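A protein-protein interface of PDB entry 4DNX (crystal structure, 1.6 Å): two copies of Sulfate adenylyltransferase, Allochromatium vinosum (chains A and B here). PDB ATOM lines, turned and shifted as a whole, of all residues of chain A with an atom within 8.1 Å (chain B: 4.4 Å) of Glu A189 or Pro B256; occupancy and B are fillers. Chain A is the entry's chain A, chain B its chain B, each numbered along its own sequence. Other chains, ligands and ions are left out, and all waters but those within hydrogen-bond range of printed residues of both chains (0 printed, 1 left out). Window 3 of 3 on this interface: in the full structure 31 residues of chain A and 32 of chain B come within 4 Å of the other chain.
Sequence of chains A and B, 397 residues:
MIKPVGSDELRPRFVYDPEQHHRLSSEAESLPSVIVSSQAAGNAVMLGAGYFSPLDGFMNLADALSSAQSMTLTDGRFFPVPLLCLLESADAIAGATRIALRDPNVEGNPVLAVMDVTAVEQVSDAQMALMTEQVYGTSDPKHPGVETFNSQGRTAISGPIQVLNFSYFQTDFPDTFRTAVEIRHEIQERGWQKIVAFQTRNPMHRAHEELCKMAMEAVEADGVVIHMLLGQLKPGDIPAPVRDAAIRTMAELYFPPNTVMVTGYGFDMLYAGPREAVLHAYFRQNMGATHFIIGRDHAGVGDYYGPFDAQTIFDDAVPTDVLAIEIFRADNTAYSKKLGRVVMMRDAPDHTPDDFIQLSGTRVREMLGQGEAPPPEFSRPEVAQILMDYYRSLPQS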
ATOM      1  N   MET A   1     -35.508  -2.385 -17.283  1.00  0.00           N
ATOM      2  CA  MET A   1     -36.199  -1.113 -17.634  1.00  0.00           C
ATOM      3  C   MET A   1     -37.427  -1.457 -18.477  1.00  0.00           C
ATOM      4  O   MET A   1     -37.410  -2.435 -19.223  1.00  0.00           O
ATOM      5  CB  MET A   1     -35.222  -0.180 -18.382  1.00  0.00           C
ATOM      6  CG  MET A   1     -35.746   1.242 -18.711  1.00  0.00           C
ATOM      7  SD  MET A   1     -34.852   2.566 -17.833  1.00  0.00           S
ATOM      8  CE  MET A   1     -34.509   1.676 -16.339  1.00  0.00           C
ATOM      9  N   GLU A 182     -31.947  10.724 -21.810  1.00  0.00           N
ATOM     10  CA  GLU A 182     -31.155  10.987 -20.585  1.00  0.00           C
ATOM     11  C   GLU A 182     -31.953  10.613 -19.328  1.00  0.00           C
ATOM     12  O   GLU A 182     -31.337  10.133 -18.351  1.00  0.00           O
ATOM     13  CB  GLU A 182     -30.734  12.452 -20.532  1.00  0.00           C
ATOM     14  CG  GLU A 182     -29.807  12.834 -19.319  1.00  0.00           C
ATOM     15  CD  GLU A 182     -28.519  11.971 -19.153  1.00  0.00           C
ATOM     16  OE1 GLU A 182     -28.058  11.287 -20.103  1.00  0.00           O
ATOM     17  OE2 GLU A 182     -27.926  12.027 -18.039  1.00  0.00           O
ATOM     18  N   ILE A 183     -33.269  10.810 -19.354  1.00  0.00           N
ATOM     19  CA  ILE A 183     -34.098  10.377 -18.180  1.00  0.00           C
ATOM     20  C   ILE A 183     -33.971   8.853 -18.018  1.00  0.00           C
ATOM     21  O   ILE A 183     -33.732   8.351 -16.879  1.00  0.00           O
ATOM     22  CB  ILE A 183     -35.531  10.816 -18.356  1.00  0.00           C
ATOM     23  CG1 ILE A 183     -35.600  12.336 -18.189  1.00  0.00           C
ATOM     24  CG2 ILE A 183     -36.425  10.148 -17.360  1.00  0.00           C
ATOM     25  CD1 ILE A 183     -37.001  12.970 -18.479  1.00  0.00           C
ATOM     26  N   ARG A 184     -34.078   8.093 -19.138  1.00  0.00           N
ATOM     27  CA  ARG A 184     -33.886   6.620 -19.085  1.00  0.00           C
ATOM     28  C   ARG A 184     -32.496   6.230 -18.517  1.00  0.00           C
ATOM     29  O   ARG A 184     -32.401   5.324 -17.670  1.00  0.00           O
ATOM     30  CB  ARG A 184     -34.151   6.016 -20.519  1.00  0.00           C
ATOM     31  CG  ARG A 184     -34.187   4.496 -20.722  1.00  0.00           C
ATOM     32  CD  ARG A 184     -34.794   4.251 -22.147  1.00  0.00           C
ATOM     33  NE  ARG A 184     -36.281   4.152 -22.151  1.00  0.00           N
ATOM     34  CZ  ARG A 184     -36.932   3.012 -21.910  1.00  0.00           C
ATOM     35  NH1 ARG A 184     -36.255   1.879 -21.596  1.00  0.00           N
ATOM     36  NH2 ARG A 184     -38.257   2.979 -21.901  1.00  0.00           N
ATOM     37  N   HIS A 185     -31.429   6.920 -18.938  1.00  0.00           N
ATOM     38  CA  HIS A 185     -30.071   6.630 -18.429  1.00  0.00           C
ATOM     39  C   HIS A 185     -29.999   6.854 -16.927  1.00  0.00           C
ATOM     40  O   HIS A 185     -29.460   5.998 -16.212  1.00  0.00           O
ATOM     41  CB  HIS A 185     -29.056   7.560 -19.100  1.00  0.00           C
ATOM     42  CG  HIS A 185     -28.742   7.193 -20.516  1.00  0.00           C
ATOM     43  ND1 HIS A 185     -28.389   8.136 -21.468  1.00  0.00           N
ATOM     44  CD2 HIS A 185     -28.769   6.008 -21.159  1.00  0.00           C
ATOM     45  CE1 HIS A 185     -28.183   7.532 -22.622  1.00  0.00           C
ATOM     46  NE2 HIS A 185     -28.386   6.242 -22.462  1.00  0.00           N
ATOM     47  N   GLU A 186     -30.524   8.004 -16.484  1.00  0.00           N
ATOM     48  CA  GLU A 186     -30.508   8.366 -15.060  1.00  0.00           C
ATOM     49  C   GLU A 186     -31.342   7.428 -14.179  1.00  0.00           C
ATOM     50  O   GLU A 186     -30.894   7.069 -13.084  1.00  0.00           O
ATOM     51  CB  GLU A 186     -30.931   9.812 -14.854  1.00  0.00           C
ATOM     52  CG  GLU A 186     -31.037  10.234 -13.392  1.00  0.00           C
ATOM     53  CD  GLU A 186     -30.890  11.737 -13.182  1.00  0.00           C
ATOM     54  OE1 GLU A 186     -30.762  12.124 -12.001  1.00  0.00           O
ATOM     55  OE2 GLU A 186     -30.897  12.522 -14.186  1.00  0.00           O
ATOM     56  N   ILE A 187     -32.533   7.029 -14.638  1.00  0.00           N
ATOM     57  CA  ILE A 187     -33.332   6.009 -13.892  1.00  0.00           C
ATOM     58  C   ILE A 187     -32.492   4.747 -13.731  1.00  0.00           C
ATOM     59  O   ILE A 187     -32.434   4.120 -12.645  1.00  0.00           O
ATOM     60  CB  ILE A 187     -34.658   5.683 -14.618  1.00  0.00           C
ATOM     61  CG1 ILE A 187     -35.622   6.869 -14.457  1.00  0.00           C
ATOM     62  CG2 ILE A 187     -35.264   4.375 -14.071  1.00  0.00           C
ATOM     63  CD1 ILE A 187     -36.869   6.813 -15.371  1.00  0.00           C
ATOM     64  N   GLN A 188     -31.794   4.392 -14.804  1.00  0.00           N
ATOM     65  CA  GLN A 188     -31.059   3.144 -14.848  1.00  0.00           C
ATOM     66  C   GLN A 188     -29.995   3.140 -13.810  1.00  0.00           C
ATOM     67  O   GLN A 188     -29.852   2.182 -13.008  1.00  0.00           O
ATOM     68  CB  GLN A 188     -30.393   3.004 -16.209  1.00  0.00           C
ATOM     69  CG  GLN A 188     -31.170   2.172 -17.104  1.00  0.00           C
ATOM     70  CD  GLN A 188     -30.637   0.776 -17.149  1.00  0.00           C
ATOM     71  OE1 GLN A 188     -30.156   0.249 -16.136  1.00  0.00           O
ATOM     72  NE2 GLN A 188     -30.707   0.161 -18.326  1.00  0.00           N
ATOM     73  N   GLU A 189     -29.240   4.216 -13.786  1.00  0.00           N
ATOM     74  CA  GLU A 189     -28.094   4.202 -12.942  1.00  0.00           C
ATOM     75  C   GLU A 189     -28.472   4.358 -11.473  1.00  0.00           C
ATOM     76  O   GLU A 189     -27.838   3.721 -10.616  1.00  0.00           O
ATOM     77  CB  GLU A 189     -27.064   5.234 -13.390  1.00  0.00           C
ATOM     78  CG  GLU A 189     -25.662   4.912 -12.859  1.00  0.00           C
ATOM     79  CD  GLU A 189     -25.588   5.179 -11.369  1.00  0.00           C
ATOM     80  OE1 GLU A 189     -26.311   6.137 -10.968  1.00  0.00           O
ATOM     81  OE2 GLU A 189     -24.900   4.455 -10.603  1.00  0.00           O
ATOM     82  N   ARG A 190     -29.533   5.133 -11.202  1.00  0.00           N
ATOM     83  CA  ARG A 190     -29.973   5.377  -9.813  1.00  0.00           C
ATOM     84  C   ARG A 190     -30.531   4.086  -9.199  1.00  0.00           C
ATOM     85  O   ARG A 190     -30.778   3.997  -7.979  1.00  0.00           O
ATOM     86  CB  ARG A 190     -31.015   6.496  -9.794  1.00  0.00           C
ATOM     87  CG  ARG A 190     -30.468   7.934  -9.948  1.00  0.00           C
ATOM     88  CD  ARG A 190     -31.607   8.768  -9.514  1.00  0.00           C
ATOM     89  NE  ARG A 190     -31.563  10.185  -9.770  1.00  0.00           N
ATOM     90  CZ  ARG A 190     -32.068  11.054  -8.922  1.00  0.00           C
ATOM     91  NH1 ARG A 190     -32.573  10.639  -7.733  1.00  0.00           N
ATOM     92  NH2 ARG A 190     -31.991  12.333  -9.204  1.00  0.00           N
ATOM     93  N   GLY A 191     -30.728   3.080 -10.036  1.00  0.00           N
ATOM     94  CA  GLY A 191     -31.173   1.738  -9.585  1.00  0.00           C
ATOM     95  C   GLY A 191     -32.670   1.511  -9.430  1.00  0.00           C
ATOM     96  O   GLY A 191     -33.103   0.481  -8.879  1.00  0.00           O
ATOM     97  N   TRP A 192     -33.472   2.484  -9.872  1.00  0.00           N
ATOM     98  CA  TRP A 192     -34.930   2.409  -9.708  1.00  0.00           C
ATOM     99  C   TRP A 192     -35.538   1.351 -10.637  1.00  0.00           C
ATOM    100  O   TRP A 192     -35.220   1.348 -11.856  1.00  0.00           O
ATOM    101  CB  TRP A 192     -35.561   3.763 -10.032  1.00  0.00           C
ATOM    102  CG  TRP A 192     -35.193   4.868  -9.081  1.00  0.00           C
ATOM    103  CD1 TRP A 192     -34.453   4.784  -7.907  1.00  0.00           C
ATOM    104  CD2 TRP A 192     -35.583   6.227  -9.218  1.00  0.00           C
ATOM    105  NE1 TRP A 192     -34.352   6.041  -7.332  1.00  0.00           N
ATOM    106  CE2 TRP A 192     -35.059   6.937  -8.098  1.00  0.00           C
ATOM    107  CE3 TRP A 192     -36.330   6.932 -10.195  1.00  0.00           C
ATOM    108  CZ2 TRP A 192     -35.262   8.329  -7.924  1.00  0.00           C
ATOM    109  CZ3 TRP A 192     -36.535   8.334 -10.008  1.00  0.00           C
ATOM    110  CH2 TRP A 192     -36.010   8.996  -8.894  1.00  0.00           C
ATOM    111  N   ASN A 258     -32.486   9.726  -2.688  1.00  0.00           N
ATOM    112  CA  ASN A 258     -32.589   9.030  -3.974  1.00  0.00           C
ATOM    113  C   ASN A 258     -34.019   8.566  -4.312  1.00  0.00           C
ATOM    114  O   ASN A 258     -34.242   7.392  -4.679  1.00  0.00           O
ATOM    115  CB  ASN A 258     -31.601   7.845  -4.025  1.00  0.00           C
ATOM    116  CG  ASN A 258     -31.494   7.277  -5.455  1.00  0.00           C
ATOM    117  OD1 ASN A 258     -31.609   8.052  -6.422  1.00  0.00           O
ATOM    118  ND2 ASN A 258     -31.321   5.957  -5.594  1.00  0.00           N
ATOM    119  N   ARG B 190     -29.541  12.466  -5.005  1.00  0.00           N
ATOM    120  CA  ARG B 190     -29.061  11.103  -4.877  1.00  0.00           C
ATOM    121  C   ARG B 190     -28.656  10.761  -3.421  1.00  0.00           C
ATOM    122  O   ARG B 190     -28.494   9.559  -3.088  1.00  0.00           O
ATOM    123  CB  ARG B 190     -27.925  10.888  -5.843  1.00  0.00           C
ATOM    124  CG  ARG B 190     -28.325  10.800  -7.372  1.00  0.00           C
ATOM    125  CD  ARG B 190     -27.046  10.691  -8.111  1.00  0.00           C
ATOM    126  NE  ARG B 190     -27.129  10.500  -9.552  1.00  0.00           N
ATOM    127  CZ  ARG B 190     -26.807   9.373 -10.157  1.00  0.00           C
ATOM    128  NH1 ARG B 190     -26.457   8.273  -9.465  1.00  0.00           N
ATOM    129  NH2 ARG B 190     -26.889   9.333 -11.481  1.00  0.00           N
ATOM    130  N   PHE B 255     -20.758  -1.022 -11.539  1.00  0.00           N
ATOM    131  CA  PHE B 255     -20.846  -0.267 -10.296  1.00  0.00           C
ATOM    132  C   PHE B 255     -22.168  -0.548  -9.607  1.00  0.00           C
ATOM    133  O   PHE B 255     -23.174  -0.810 -10.284  1.00  0.00           O
ATOM    134  CB  PHE B 255     -20.732   1.217 -10.583  1.00  0.00           C
ATOM    135  CG  PHE B 255     -19.306   1.675 -10.835  1.00  0.00           C
ATOM    136  CD1 PHE B 255     -18.676   1.452 -12.079  1.00  0.00           C
ATOM    137  CD2 PHE B 255     -18.583   2.306  -9.819  1.00  0.00           C
ATOM    138  CE1 PHE B 255     -17.345   1.908 -12.313  1.00  0.00           C
ATOM    139  CE2 PHE B 255     -17.265   2.771 -10.025  1.00  0.00           C
ATOM    140  CZ  PHE B 255     -16.626   2.561 -11.290  1.00  0.00           C
ATOM    141  N   PRO B 256     -22.209  -0.488  -8.274  1.00  0.00           N
ATOM    142  CA  PRO B 256     -23.476  -0.682  -7.602  1.00  0.00           C
ATOM    143  C   PRO B 256     -24.524   0.388  -7.968  1.00  0.00           C
ATOM    144  O   PRO B 256     -24.194   1.482  -8.444  1.00  0.00           O
ATOM    145  CB  PRO B 256     -23.130  -0.486  -6.086  1.00  0.00           C
ATOM    146  CG  PRO B 256     -21.718  -0.702  -5.978  1.00  0.00           C
ATOM    147  CD  PRO B 256     -21.133  -0.179  -7.302  1.00  0.00           C
ATOM    148  N   PRO B 257     -25.785   0.095  -7.671  1.00  0.00           N
ATOM    149  CA  PRO B 257     -26.853   1.074  -7.891  1.00  0.00           C
ATOM    150  C   PRO B 257     -26.589   2.430  -7.235  1.00  0.00           C
ATOM    151  O   PRO B 257     -26.159   2.497  -6.064  1.00  0.00           O
ATOM    152  CB  PRO B 257     -28.071   0.440  -7.197  1.00  0.00           C
ATOM    153  CG  PRO B 257     -27.711  -1.006  -6.961  1.00  0.00           C
ATOM    154  CD  PRO B 257     -26.237  -1.056  -6.851  1.00  0.00           C
ATOM    155  N   ASN B 258     -26.896   3.507  -7.948  1.00  0.00           N
ATOM    156  CA  ASN B 258     -26.756   4.862  -7.408  1.00  0.00           C
ATOM    157  C   ASN B 258     -25.325   5.223  -6.922  1.00  0.00           C
ATOM    158  O   ASN B 258     -25.134   5.729  -5.802  1.00  0.00           O
ATOM    159  CB  ASN B 258     -27.798   5.172  -6.299  1.00  0.00           C
ATOM    160  CG  ASN B 258     -27.832   6.636  -5.942  1.00  0.00           C
ATOM    161  OD1 ASN B 258     -27.598   7.515  -6.804  1.00  0.00           O
ATOM    162  ND2 ASN B 258     -28.105   6.935  -4.658  1.00  0.00           N
ATOM    163  N   THR B 259     -24.338   4.904  -7.748  1.00  0.00           N
ATOM    164  CA  THR B 259     -22.946   5.273  -7.422  1.00  0.00           C
ATOM    165  C   THR B 259     -22.189   6.062  -8.458  1.00  0.00           C
ATOM    166  O   THR B 259     -21.089   6.530  -8.154  1.00  0.00           O
ATOM    167  CB  THR B 259     -22.084   4.053  -6.994  1.00  0.00           C
ATOM    168  OG1 THR B 259     -21.980   3.141  -8.075  1.00  0.00           O
ATOM    169  CG2 THR B 259     -22.660   3.360  -5.752  1.00  0.00           C
ATOM    170  N   VAL B 260     -22.754   6.283  -9.658  1.00  0.00           N
ATOM    171  CA  VAL B 260     -22.005   6.979 -10.697  1.00  0.00           C
ATOM    172  C   VAL B 260     -22.875   8.033 -11.381  1.00  0.00           C
ATOM    173  O   VAL B 260     -24.011   7.739 -11.707  1.00  0.00           O
ATOM    174  CB  VAL B 260     -21.526   5.975 -11.787  1.00  0.00           C
ATOM    175  CG1 VAL B 260     -20.692   6.672 -12.842  1.00  0.00           C
ATOM    176  CG2 VAL B 260     -20.693   4.876 -11.145  1.00  0.00           C
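Of the printed residues of chain B, Glu A189 touches Arg B190 (2.6 Å), Pro B256 (3.7 Å), Pro B257 (3.8 Å), Asn B258 (2.8 Å), Thr B259 (2.9 Å) and Val B260 (2.9 Å). Of the printed residues of chain A, Pro B256 touches Glu A189 (3.7 Å). Of the printed residues of chain A, Pro B257 touches Glu A189 (3.8 Å). Of the printed residues of chain A, Val B260 touches Glu A189. Of the printed residues of chain B, Arg A190 touches Arg B190 (3.9 Å) and Asn B258 (3.6 Å). Of the printed residues of chain A, Asn B258 touches Glu A189 (2.8 Å), Arg A190 (3.6 Å) and Asn A258 (3.5 Å). The nearest printed residue of chain B that does not touch Glu A189 is Phe B255 (5.3 Å). The nearest printed residue of chain A that does not touch Pro B256 is Arg A190 (6.9 Å). The nearest printed residue of chain B that does not touch Asn A258 is Pro B257 (6.1 Å).
The backbone NH of Val B260 sits at hydrogen-bond distance from the side-chain carboxylate of Glu A189, 3.0 Å away. The side-chain carboxylate (OE1) of Glu A189 lies within salt-bridge range of the guanidinium group (NH1) of Arg B190, at 2.6 Å. The backbone carbonyl oxygen of Glu A189 is in hydrogen-bond range of the backbone NH of Asn B258 (2.8 Å). The side-chain amide nitrogen (ND2) of Asn A258 lies close to the side-chain amide nitrogen (ND2) of Asn B258 (3.5 Å). The side-chain carboxylate of Glu A189 lies within hydrogen-bond range of the backbone NH of Thr B259.
Of the 13 printed residues of chain A, 3 touch a printed residue of chain B. Printed residues of chain A that touch a printed residue of chain B: Glu A189, Arg A190 and Asn A258. Hydrophobic or aromatic side chains of chain B within 4 Å of the printed part of chain A: Val B260.
Arg B190 touches its own counterpart, Arg A190. Arg A190 touches Asn B258, and with the chains exchanged Asn A258 touches Arg B190. Asn A258 touches its own counterpart, Asn B258. Of the 10 pairs that touch across the chains among the printed residues, 4 have their exchanged pair printed and touching as well.
Among the printed residues, pairs that only touch across the chains: Arg A190 with Asn B258 (3.6 Å), Asn A258 with Arg B190 (3.7 Å), Glu A189 with Pro B256 (3.7 Å), Glu A189 with Pro B257 (3.8 Å) and Arg A190 with Arg B190 (3.9 Å).
OD1 of Asn A258 sits at hydrogen-bond distance from NH1 of Arg A190. The side-chain carboxylate of Glu A186 is in salt-bridge range of the guanidinium group of Arg A190, at 3.1 Å. The backbone carbonyl oxygen (O) of Pro B256 lies within hydrogen-bond range of the side-chain hydroxyl (OG1) of Thr B259 (2.8 Å). The side-chain amide oxygen (OD1) of Asn B258 sits at hydrogen-bond distance from the guanidinium group (NH1) of Arg B190 (3.0 Å). The backbone carbonyl oxygen (O) of Val B260 sits at hydrogen-bond distance from the guanidinium group (NH2) of Arg B190, 3.3 Å away. NE1 of Trp A192 sits at hydrogen-bond distance from O of Asn A258 (3.0 Å).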
